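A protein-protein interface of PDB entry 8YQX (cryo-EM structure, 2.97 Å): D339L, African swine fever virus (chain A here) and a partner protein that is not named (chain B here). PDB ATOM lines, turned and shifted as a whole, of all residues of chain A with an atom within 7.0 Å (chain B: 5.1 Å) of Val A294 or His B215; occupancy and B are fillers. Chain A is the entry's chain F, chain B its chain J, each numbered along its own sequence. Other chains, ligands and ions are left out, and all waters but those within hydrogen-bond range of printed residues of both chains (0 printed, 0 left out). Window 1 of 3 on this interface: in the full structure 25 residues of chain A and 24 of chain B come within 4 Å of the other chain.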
ATOM      1  N   ASN A  82     -14.235  -9.464  41.571  1.00  0.00           N
ATOM      2  CA  ASN A  82     -15.323  -8.976  40.740  1.00  0.00           C
ATOM      3  C   ASN A  82     -16.636  -9.636  41.140  1.00  0.00           C
ATOM      4  O   ASN A  82     -16.684 -10.524  41.994  1.00  0.00           O
ATOM      5  CB  ASN A  82     -15.027  -9.238  39.260  1.00  0.00           C
ATOM      6  CG  ASN A  82     -13.777  -8.530  38.784  1.00  0.00           C
ATOM      7  OD1 ASN A  82     -13.734  -7.304  38.716  1.00  0.00           O
ATOM      8  ND2 ASN A  82     -12.748  -9.302  38.458  1.00  0.00           N
ATOM      9  N   LEU A 178      -5.894 -11.673  23.984  1.00  0.00           N
ATOM     10  CA  LEU A 178      -6.581 -12.822  24.564  1.00  0.00           C
ATOM     11  C   LEU A 178      -5.667 -14.025  24.737  1.00  0.00           C
ATOM     12  O   LEU A 178      -6.016 -14.953  25.478  1.00  0.00           O
ATOM     13  CB  LEU A 178      -7.780 -13.209  23.701  1.00  0.00           C
ATOM     14  CG  LEU A 178      -8.880 -12.155  23.616  1.00  0.00           C
ATOM     15  CD1 LEU A 178     -10.031 -12.651  22.767  1.00  0.00           C
ATOM     16  CD2 LEU A 178      -9.351 -11.787  25.005  1.00  0.00           C
ATOM     17  N   LEU A 181      -5.051 -14.568  28.432  1.00  0.00           N
ATOM     18  CA  LEU A 181      -6.071 -15.362  29.108  1.00  0.00           C
ATOM     19  C   LEU A 181      -5.986 -16.826  28.705  1.00  0.00           C
ATOM     20  O   LEU A 181      -6.239 -17.715  29.526  1.00  0.00           O
ATOM     21  CB  LEU A 181      -7.463 -14.808  28.804  1.00  0.00           C
ATOM     22  CG  LEU A 181      -7.798 -13.436  29.390  1.00  0.00           C
ATOM     23  CD1 LEU A 181      -9.173 -12.978  28.931  1.00  0.00           C
ATOM     24  CD2 LEU A 181      -7.721 -13.471  30.904  1.00  0.00           C
ATOM     25  N   ALA A 289     -16.727 -10.034  18.693  1.00  0.00           N
ATOM     26  CA  ALA A 289     -16.103 -11.310  19.027  1.00  0.00           C
ATOM     27  C   ALA A 289     -15.228 -11.186  20.265  1.00  0.00           C
ATOM     28  O   ALA A 289     -15.174 -12.107  21.090  1.00  0.00           O
ATOM     29  CB  ALA A 289     -15.284 -11.820  17.843  1.00  0.00           C
ATOM     30  N   GLU A 290     -14.535 -10.057  20.410  1.00  0.00           N
ATOM     31  CA  GLU A 290     -13.630  -9.876  21.537  1.00  0.00           C
ATOM     32  C   GLU A 290     -14.380  -9.847  22.863  1.00  0.00           C
ATOM     33  O   GLU A 290     -13.907 -10.419  23.850  1.00  0.00           O
ATOM     34  CB  GLU A 290     -12.818  -8.598  21.342  1.00  0.00           C
ATOM     35  CG  GLU A 290     -11.568  -8.513  22.191  1.00  0.00           C
ATOM     36  CD  GLU A 290     -11.802  -7.820  23.508  1.00  0.00           C
ATOM     37  OE1 GLU A 290     -12.755  -7.020  23.600  1.00  0.00           O
ATOM     38  OE2 GLU A 290     -11.025  -8.069  24.449  1.00  0.00           O
ATOM     39  N   VAL A 291     -15.552  -9.207  22.904  1.00  0.00           N
ATOM     40  CA  VAL A 291     -16.335  -9.146  24.139  1.00  0.00           C
ATOM     41  C   VAL A 291     -16.794 -10.540  24.554  1.00  0.00           C
ATOM     42  O   VAL A 291     -16.649 -10.946  25.716  1.00  0.00           O
ATOM     43  CB  VAL A 291     -17.530  -8.192  23.963  1.00  0.00           C
ATOM     44  CG1 VAL A 291     -18.532  -8.370  25.091  1.00  0.00           C
ATOM     45  CG2 VAL A 291     -17.050  -6.753  23.887  1.00  0.00           C
ATOM     46  N   MET A 292     -17.358 -11.293  23.605  1.00  0.00           N
ATOM     47  CA  MET A 292     -17.828 -12.639  23.913  1.00  0.00           C
ATOM     48  C   MET A 292     -16.674 -13.527  24.348  1.00  0.00           C
ATOM     49  O   MET A 292     -16.805 -14.318  25.290  1.00  0.00           O
ATOM     50  CB  MET A 292     -18.526 -13.247  22.696  1.00  0.00           C
ATOM     51  CG  MET A 292     -18.658 -14.764  22.749  1.00  0.00           C
ATOM     52  SD  MET A 292     -17.402 -15.665  21.819  1.00  0.00           S
ATOM     53  CE  MET A 292     -17.319 -14.714  20.309  1.00  0.00           C
ATOM     54  N   PHE A 293     -15.535 -13.415  23.661  1.00  0.00           N
ATOM     55  CA  PHE A 293     -14.380 -14.232  24.010  1.00  0.00           C
ATOM     56  C   PHE A 293     -13.856 -13.885  25.395  1.00  0.00           C
ATOM     57  O   PHE A 293     -13.499 -14.779  26.166  1.00  0.00           O
ATOM     58  CB  PHE A 293     -13.288 -14.070  22.954  1.00  0.00           C
ATOM     59  CG  PHE A 293     -13.391 -15.055  21.828  1.00  0.00           C
ATOM     60  CD1 PHE A 293     -14.004 -16.282  22.021  1.00  0.00           C
ATOM     61  CD2 PHE A 293     -12.892 -14.752  20.575  1.00  0.00           C
ATOM     62  CE1 PHE A 293     -14.109 -17.190  20.989  1.00  0.00           C
ATOM     63  CE2 PHE A 293     -12.993 -15.658  19.537  1.00  0.00           C
ATOM     64  CZ  PHE A 293     -13.603 -16.878  19.745  1.00  0.00           C
ATOM     65  N   VAL A 294     -13.817 -12.595  25.737  1.00  0.00           N
ATOM     66  CA  VAL A 294     -13.392 -12.194  27.076  1.00  0.00           C
ATOM     67  C   VAL A 294     -14.322 -12.789  28.124  1.00  0.00           C
ATOM     68  O   VAL A 294     -13.873 -13.358  29.128  1.00  0.00           O
ATOM     69  CB  VAL A 294     -13.335 -10.658  27.183  1.00  0.00           C
ATOM     70  CG1 VAL A 294     -13.497 -10.215  28.626  1.00  0.00           C
ATOM     71  CG2 VAL A 294     -12.033 -10.142  26.626  1.00  0.00           C
ATOM     72  N   THR A 295     -15.633 -12.679  27.897  1.00  0.00           N
ATOM     73  CA  THR A 295     -16.595 -13.199  28.865  1.00  0.00           C
ATOM     74  C   THR A 295     -16.433 -14.705  29.048  1.00  0.00           C
ATOM     75  O   THR A 295     -16.366 -15.202  30.180  1.00  0.00           O
ATOM     76  CB  THR A 295     -18.019 -12.864  28.423  1.00  0.00           C
ATOM     77  OG1 THR A 295     -18.126 -11.456  28.179  1.00  0.00           O
ATOM     78  CG2 THR A 295     -19.016 -13.263  29.498  1.00  0.00           C
ATOM     79  N   LEU A 296     -16.353 -15.447  27.941  1.00  0.00           N
ATOM     80  CA  LEU A 296     -16.253 -16.900  28.032  1.00  0.00           C
ATOM     81  C   LEU A 296     -14.932 -17.333  28.658  1.00  0.00           C
ATOM     82  O   LEU A 296     -14.903 -18.258  29.481  1.00  0.00           O
ATOM     83  CB  LEU A 296     -16.426 -17.529  26.650  1.00  0.00           C
ATOM     84  CG  LEU A 296     -17.757 -17.291  25.932  1.00  0.00           C
ATOM     85  CD1 LEU A 296     -17.982 -18.347  24.862  1.00  0.00           C
ATOM     86  CD2 LEU A 296     -18.920 -17.260  26.913  1.00  0.00           C
ATOM     87  N   LEU A 297     -13.827 -16.681  28.285  1.00  0.00           N
ATOM     88  CA  LEU A 297     -12.532 -17.031  28.854  1.00  0.00           C
ATOM     89  C   LEU A 297     -12.504 -16.769  30.351  1.00  0.00           C
ATOM     90  O   LEU A 297     -11.987 -17.587  31.121  1.00  0.00           O
ATOM     91  CB  LEU A 297     -11.419 -16.253  28.153  1.00  0.00           C
ATOM     92  CG  LEU A 297     -11.082 -16.642  26.711  1.00  0.00           C
ATOM     93  CD1 LEU A 297      -9.851 -15.892  26.223  1.00  0.00           C
ATOM     94  CD2 LEU A 297     -10.898 -18.139  26.565  1.00  0.00           C
ATOM     95  N   LYS A 298     -13.057 -15.635  30.791  1.00  0.00           N
ATOM     96  CA  LYS A 298     -13.061 -15.358  32.222  1.00  0.00           C
ATOM     97  C   LYS A 298     -13.996 -16.297  32.973  1.00  0.00           C
ATOM     98  O   LYS A 298     -13.709 -16.660  34.117  1.00  0.00           O
ATOM     99  CB  LYS A 298     -13.430 -13.900  32.489  1.00  0.00           C
ATOM    100  CG  LYS A 298     -13.336 -13.533  33.959  1.00  0.00           C
ATOM    101  CD  LYS A 298     -12.406 -12.358  34.191  1.00  0.00           C
ATOM    102  CE  LYS A 298     -12.320 -12.019  35.671  1.00  0.00           C
ATOM    103  NZ  LYS A 298     -11.965 -13.211  36.490  1.00  0.00           N
ATOM    104  N   GLU A 299     -15.108 -16.710  32.357  1.00  0.00           N
ATOM    105  CA  GLU A 299     -15.964 -17.705  33.000  1.00  0.00           C
ATOM    106  C   GLU A 299     -15.240 -19.037  33.156  1.00  0.00           C
ATOM    107  O   GLU A 299     -15.337 -19.691  34.204  1.00  0.00           O
ATOM    108  CB  GLU A 299     -17.254 -17.884  32.200  1.00  0.00           C
ATOM    109  CG  GLU A 299     -18.464 -18.251  33.044  1.00  0.00           C
ATOM    110  CD  GLU A 299     -19.124 -17.043  33.685  1.00  0.00           C
ATOM    111  OE1 GLU A 299     -18.464 -16.354  34.491  1.00  0.00           O
ATOM    112  OE2 GLU A 299     -20.308 -16.784  33.383  1.00  0.00           O
ATOM    113  N   ILE A 300     -14.503 -19.454  32.123  1.00  0.00           N
ATOM    114  CA  ILE A 300     -13.725 -20.687  32.214  1.00  0.00           C
ATOM    115  C   ILE A 300     -12.668 -20.566  33.304  1.00  0.00           C
ATOM    116  O   ILE A 300     -12.452 -21.501  34.085  1.00  0.00           O
ATOM    117  CB  ILE A 300     -13.098 -21.031  30.850  1.00  0.00           C
ATOM    118  CG1 ILE A 300     -14.185 -21.345  29.823  1.00  0.00           C
ATOM    119  CG2 ILE A 300     -12.147 -22.208  30.980  1.00  0.00           C
ATOM    120  CD1 ILE A 300     -13.681 -21.383  28.397  1.00  0.00           C
ATOM    121  N   ILE A 301     -11.994 -19.416  33.373  1.00  0.00           N
ATOM    122  CA  ILE A 301     -11.001 -19.183  34.420  1.00  0.00           C
ATOM    123  C   ILE A 301     -11.647 -19.295  35.794  1.00  0.00           C
ATOM    124  O   ILE A 301     -11.118 -19.949  36.701  1.00  0.00           O
ATOM    125  CB  ILE A 301     -10.334 -17.810  34.230  1.00  0.00           C
ATOM    126  CG1 ILE A 301      -9.373 -17.835  33.044  1.00  0.00           C
ATOM    127  CG2 ILE A 301      -9.607 -17.386  35.495  1.00  0.00           C
ATOM    128  CD1 ILE A 301      -8.896 -16.469  32.619  1.00  0.00           C
ATOM    129  N   PRO B 153     -13.082   0.169  37.437  1.00  0.00           N
ATOM    130  CA  PRO B 153     -13.043  -0.301  36.043  1.00  0.00           C
ATOM    131  C   PRO B 153     -14.197   0.205  35.197  1.00  0.00           C
ATOM    132  O   PRO B 153     -14.025   0.394  33.987  1.00  0.00           O
ATOM    133  CB  PRO B 153     -13.078  -1.829  36.191  1.00  0.00           C
ATOM    134  CG  PRO B 153     -12.491  -2.083  37.533  1.00  0.00           C
ATOM    135  CD  PRO B 153     -12.934  -0.939  38.398  1.00  0.00           C
ATOM    136  N   GLY B 157     -13.023   1.964  31.775  1.00  0.00           N
ATOM    137  CA  GLY B 157     -13.454   1.453  30.486  1.00  0.00           C
ATOM    138  C   GLY B 157     -14.306   2.443  29.721  1.00  0.00           C
ATOM    139  O   GLY B 157     -14.202   2.549  28.497  1.00  0.00           O
ATOM    140  N   TYR B 158     -15.162   3.184  30.430  1.00  0.00           N
ATOM    141  CA  TYR B 158     -15.968   4.213  29.785  1.00  0.00           C
ATOM    142  C   TYR B 158     -15.084   5.273  29.138  1.00  0.00           C
ATOM    143  O   TYR B 158     -15.297   5.658  27.982  1.00  0.00           O
ATOM    144  CB  TYR B 158     -16.914   4.842  30.808  1.00  0.00           C
ATOM    145  CG  TYR B 158     -17.651   6.067  30.316  1.00  0.00           C
ATOM    146  CD1 TYR B 158     -18.770   5.948  29.504  1.00  0.00           C
ATOM    147  CD2 TYR B 158     -17.234   7.342  30.672  1.00  0.00           C
ATOM    148  CE1 TYR B 158     -19.448   7.065  29.055  1.00  0.00           C
ATOM    149  CE2 TYR B 158     -17.903   8.464  30.227  1.00  0.00           C
ATOM    150  CZ  TYR B 158     -19.010   8.319  29.421  1.00  0.00           C
ATOM    151  OH  TYR B 158     -19.681   9.434  28.977  1.00  0.00           O
ATOM    152  N   PHE B 168     -15.864  -0.699  23.119  1.00  0.00           N
ATOM    153  CA  PHE B 168     -16.976  -1.451  23.693  1.00  0.00           C
ATOM    154  C   PHE B 168     -18.284  -0.679  23.589  1.00  0.00           C
ATOM    155  O   PHE B 168     -19.335  -1.259  23.284  1.00  0.00           O
ATOM    156  CB  PHE B 168     -16.673  -1.799  25.148  1.00  0.00           C
ATOM    157  CG  PHE B 168     -15.412  -2.586  25.328  1.00  0.00           C
ATOM    158  CD1 PHE B 168     -15.274  -3.833  24.749  1.00  0.00           C
ATOM    159  CD2 PHE B 168     -14.363  -2.079  26.073  1.00  0.00           C
ATOM    160  CE1 PHE B 168     -14.116  -4.562  24.911  1.00  0.00           C
ATOM    161  CE2 PHE B 168     -13.203  -2.804  26.238  1.00  0.00           C
ATOM    162  CZ  PHE B 168     -13.079  -4.047  25.655  1.00  0.00           C
ATOM    163  N   PHE B 209     -21.479  -5.681  31.079  1.00  0.00           N
ATOM    164  CA  PHE B 209     -20.144  -6.056  30.626  1.00  0.00           C
ATOM    165  C   PHE B 209     -19.077  -5.171  31.255  1.00  0.00           C
ATOM    166  O   PHE B 209     -18.019  -5.659  31.668  1.00  0.00           O
ATOM    167  CB  PHE B 209     -20.066  -5.983  29.102  1.00  0.00           C
ATOM    168  CG  PHE B 209     -18.691  -6.232  28.553  1.00  0.00           C
ATOM    169  CD1 PHE B 209     -18.120  -7.492  28.620  1.00  0.00           C
ATOM    170  CD2 PHE B 209     -17.968  -5.205  27.972  1.00  0.00           C
ATOM    171  CE1 PHE B 209     -16.855  -7.722  28.118  1.00  0.00           C
ATOM    172  CE2 PHE B 209     -16.703  -5.429  27.468  1.00  0.00           C
ATOM    173  CZ  PHE B 209     -16.146  -6.689  27.540  1.00  0.00           C
ATOM    174  N   LEU B 210     -19.335  -3.863  31.332  1.00  0.00           N
ATOM    175  CA  LEU B 210     -18.365  -2.957  31.940  1.00  0.00           C
ATOM    176  C   LEU B 210     -18.172  -3.251  33.421  1.00  0.00           C
ATOM    177  O   LEU B 210     -17.083  -3.026  33.961  1.00  0.00           O
ATOM    178  CB  LEU B 210     -18.796  -1.504  31.740  1.00  0.00           C
ATOM    179  CG  LEU B 210     -18.820  -0.977  30.305  1.00  0.00           C
ATOM    180  CD1 LEU B 210     -18.965   0.535  30.295  1.00  0.00           C
ATOM    181  CD2 LEU B 210     -17.575  -1.403  29.546  1.00  0.00           C
ATOM    182  N   SER B 212     -18.632  -6.378  34.589  1.00  0.00           N
ATOM    183  CA  SER B 212     -18.464  -7.821  34.670  1.00  0.00           C
ATOM    184  C   SER B 212     -17.057  -8.174  35.148  1.00  0.00           C
ATOM    185  O   SER B 212     -16.185  -7.315  35.300  1.00  0.00           O
ATOM    186  CB  SER B 212     -18.750  -8.465  33.316  1.00  0.00           C
ATOM    187  OG  SER B 212     -17.823  -8.027  32.339  1.00  0.00           O
ATOM    188  N   GLY B 213     -16.839  -9.467  35.399  1.00  0.00           N
ATOM    189  CA  GLY B 213     -15.493  -9.933  35.692  1.00  0.00           C
ATOM    190  C   GLY B 213     -14.546  -9.675  34.538  1.00  0.00           C
ATOM    191  O   GLY B 213     -13.437  -9.171  34.725  1.00  0.00           O
ATOM    192  N   GLY B 214     -14.976 -10.017  33.326  1.00  0.00           N
ATOM    193  CA  GLY B 214     -14.293  -9.528  32.148  1.00  0.00           C
ATOM    194  C   GLY B 214     -14.414  -8.022  32.028  1.00  0.00           C
ATOM    195  O   GLY B 214     -15.289  -7.394  32.627  1.00  0.00           O
ATOM    196  N   HIS B 215     -13.498  -7.438  31.255  1.00  0.00           N
ATOM    197  CA  HIS B 215     -13.296  -5.996  31.139  1.00  0.00           C
ATOM    198  C   HIS B 215     -12.702  -5.397  32.409  1.00  0.00           C
ATOM    199  O   HIS B 215     -12.342  -4.216  32.421  1.00  0.00           O
ATOM    200  CB  HIS B 215     -14.591  -5.261  30.764  1.00  0.00           C
ATOM    201  CG  HIS B 215     -14.414  -3.792  30.542  1.00  0.00           C
ATOM    202  ND1 HIS B 215     -13.861  -3.273  29.391  1.00  0.00           N
ATOM    203  CD2 HIS B 215     -14.709  -2.733  31.329  1.00  0.00           C
ATOM    204  CE1 HIS B 215     -13.828  -1.956  29.478  1.00  0.00           C
ATOM    205  NE2 HIS B 215     -14.337  -1.602  30.645  1.00  0.00           N
ATOM    206  N   SER B 216     -12.559  -6.185  33.470  1.00  0.00           N
ATOM    207  CA  SER B 216     -11.775  -5.801  34.635  1.00  0.00           C
ATOM    208  C   SER B 216     -10.346  -6.306  34.559  1.00  0.00           C
ATOM    209  O   SER B 216      -9.423  -5.606  34.977  1.00  0.00           O
ATOM    210  CB  SER B 216     -12.430  -6.321  35.918  1.00  0.00           C
ATOM    211  OG  SER B 216     -13.664  -5.668  36.159  1.00  0.00           O
ATOM    212  N   TRP B 217     -10.149  -7.516  34.032  1.00  0.00           N
ATOM    213  CA  TRP B 217      -8.809  -7.956  33.668  1.00  0.00           C
ATOM    214  C   TRP B 217      -8.274  -7.173  32.479  1.00  0.00           C
ATOM    215  O   TRP B 217      -7.062  -6.967  32.369  1.00  0.00           O
ATOM    216  CB  TRP B 217      -8.811  -9.452  33.350  1.00  0.00           C
ATOM    217  CG  TRP B 217      -7.518  -9.944  32.768  1.00  0.00           C
ATOM    218  CD1 TRP B 217      -6.433 -10.407  33.452  1.00  0.00           C
ATOM    219  CD2 TRP B 217      -7.175 -10.012  31.378  1.00  0.00           C
ATOM    220  NE1 TRP B 217      -5.437 -10.765  32.576  1.00  0.00           N
ATOM    221  CE2 TRP B 217      -5.867 -10.530  31.297  1.00  0.00           C
ATOM    222  CE3 TRP B 217      -7.846  -9.684  30.197  1.00  0.00           C
ATOM    223  CZ2 TRP B 217      -5.219 -10.730  30.080  1.00  0.00           C
ATOM    224  CZ3 TRP B 217      -7.200  -9.883  28.991  1.00  0.00           C
ATOM    225  CH2 TRP B 217      -5.901 -10.402  28.942  1.00  0.00           C
ATOM    226  N   LEU B 218      -9.159  -6.726  31.587  1.00  0.00           N
ATOM    227  CA  LEU B 218      -8.737  -6.068  30.357  1.00  0.00           C
ATOM    228  C   LEU B 218      -8.321  -4.622  30.602  1.00  0.00           C
ATOM    229  O   LEU B 218      -7.202  -4.219  30.260  1.00  0.00           O
ATOM    230  CB  LEU B 218      -9.865  -6.135  29.323  1.00  0.00           C
ATOM    231  CG  LEU B 218      -9.652  -5.408  27.995  1.00  0.00           C
ATOM    232  CD1 LEU B 218     -10.131  -6.269  26.851  1.00  0.00           C
ATOM    233  CD2 LEU B 218     -10.378  -4.073  27.988  1.00  0.00           C
ATOM    234  N   ILE B 219      -9.220  -3.820  31.180  1.00  0.00           N
ATOM    235  CA  ILE B 219      -8.930  -2.399  31.347  1.00  0.00           C
ATOM    236  C   ILE B 219      -7.764  -2.205  32.308  1.00  0.00           C
ATOM    237  O   ILE B 219      -6.915  -1.332  32.099  1.00  0.00           O
ATOM    238  CB  ILE B 219     -10.190  -1.629  31.795  1.00  0.00           C
ATOM    239  CG1 ILE B 219     -10.028  -0.138  31.502  1.00  0.00           C
ATOM    240  CG2 ILE B 219     -10.491  -1.835  33.272  1.00  0.00           C
ATOM    241  CD1 ILE B 219      -9.969   0.190  30.031  1.00  0.00           C
ATOM    242  N   ASN B 220      -7.686  -3.028  33.357  1.00  0.00           N
ATOM    243  CA  ASN B 220      -6.556  -2.941  34.275  1.00  0.00           C
ATOM    244  C   ASN B 220      -5.258  -3.321  33.578  1.00  0.00           C
ATOM    245  O   ASN B 220      -4.228  -2.662  33.767  1.00  0.00           O
ATOM    246  CB  ASN B 220      -6.799  -3.831  35.492  1.00  0.00           C
ATOM    247  CG  ASN B 220      -7.896  -3.299  36.393  1.00  0.00           C
ATOM    248  OD1 ASN B 220      -8.069  -2.087  36.529  1.00  0.00           O
ATOM    249  ND2 ASN B 220      -8.644  -4.203  37.014  1.00  0.00           N
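The side-chain amide oxygen of Asn A82 sits at hydrogen-bond distance from the side-chain hydroxyl of Ser B216 (3.0 Å).
OG1 of Thr A295 sits at hydrogen-bond distance from O of Val A291 (2.9 Å).
OG of Ser B212 lies within hydrogen-bond range of O of Phe B209.
ND2 of Asn B220 lies within hydrogen-bond range of O of Ser B216, at 2.6 Å.
OG of Ser B212 sits at hydrogen-bond distance from O of Gly B214, 2.6 Å away.
The backbone carbonyl oxygen (O) of Ser B212 lies within hydrogen-bond range of the side-chain hydroxyl (OG) of Ser B216 (3.1 Å).
Among the printed residues, merely in contact across the chains: Asn A82 with Gly B213 (3.7 Å), Leu A181 with Trp B217 (3.5 Å), Glu A290 with Phe B168 (3.1 Å), Glu A290 with Leu B218 (3.1 Å), Val A291 with Phe B168 (3.5 Å), Val A291 with Phe B209 (3.5 Å), Val A294 with Gly B214 (3.7 Å), Val A294 with His B215 (3.8 Å), Thr A295 with Phe B209 (3.9 Å), Lys A298 with Gly B213 (3.2 Å) and Lys A298 with Gly B214 (3.6 Å).
Of the printed residues of chain B, Asn A82 touches Gly B213 and Ser B216.
Leu A178 touches none of the printed residues of chain B.
Val A294 touches two residues of chain B.
His B215 touches one residue of chain A.
Printed residues of chain A within 4 Å of Ser B216: Asn A82 (3.0 Å).
The nearest printed residue of chain B that does not touch Glu A290 is Phe B209 (5.2 Å).
Of the 16 printed residues of chain A, 7 touch a printed residue of chain B.
Hydrophobic or aromatic side chains of chain A that line the printed part of chain B: Leu A181, Val A291 and Val A294.
Among the printed residues, no Asp or Glu carboxylate lies within 4 Å of a Lys or Arg side-chain nitrogen of the other chain.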
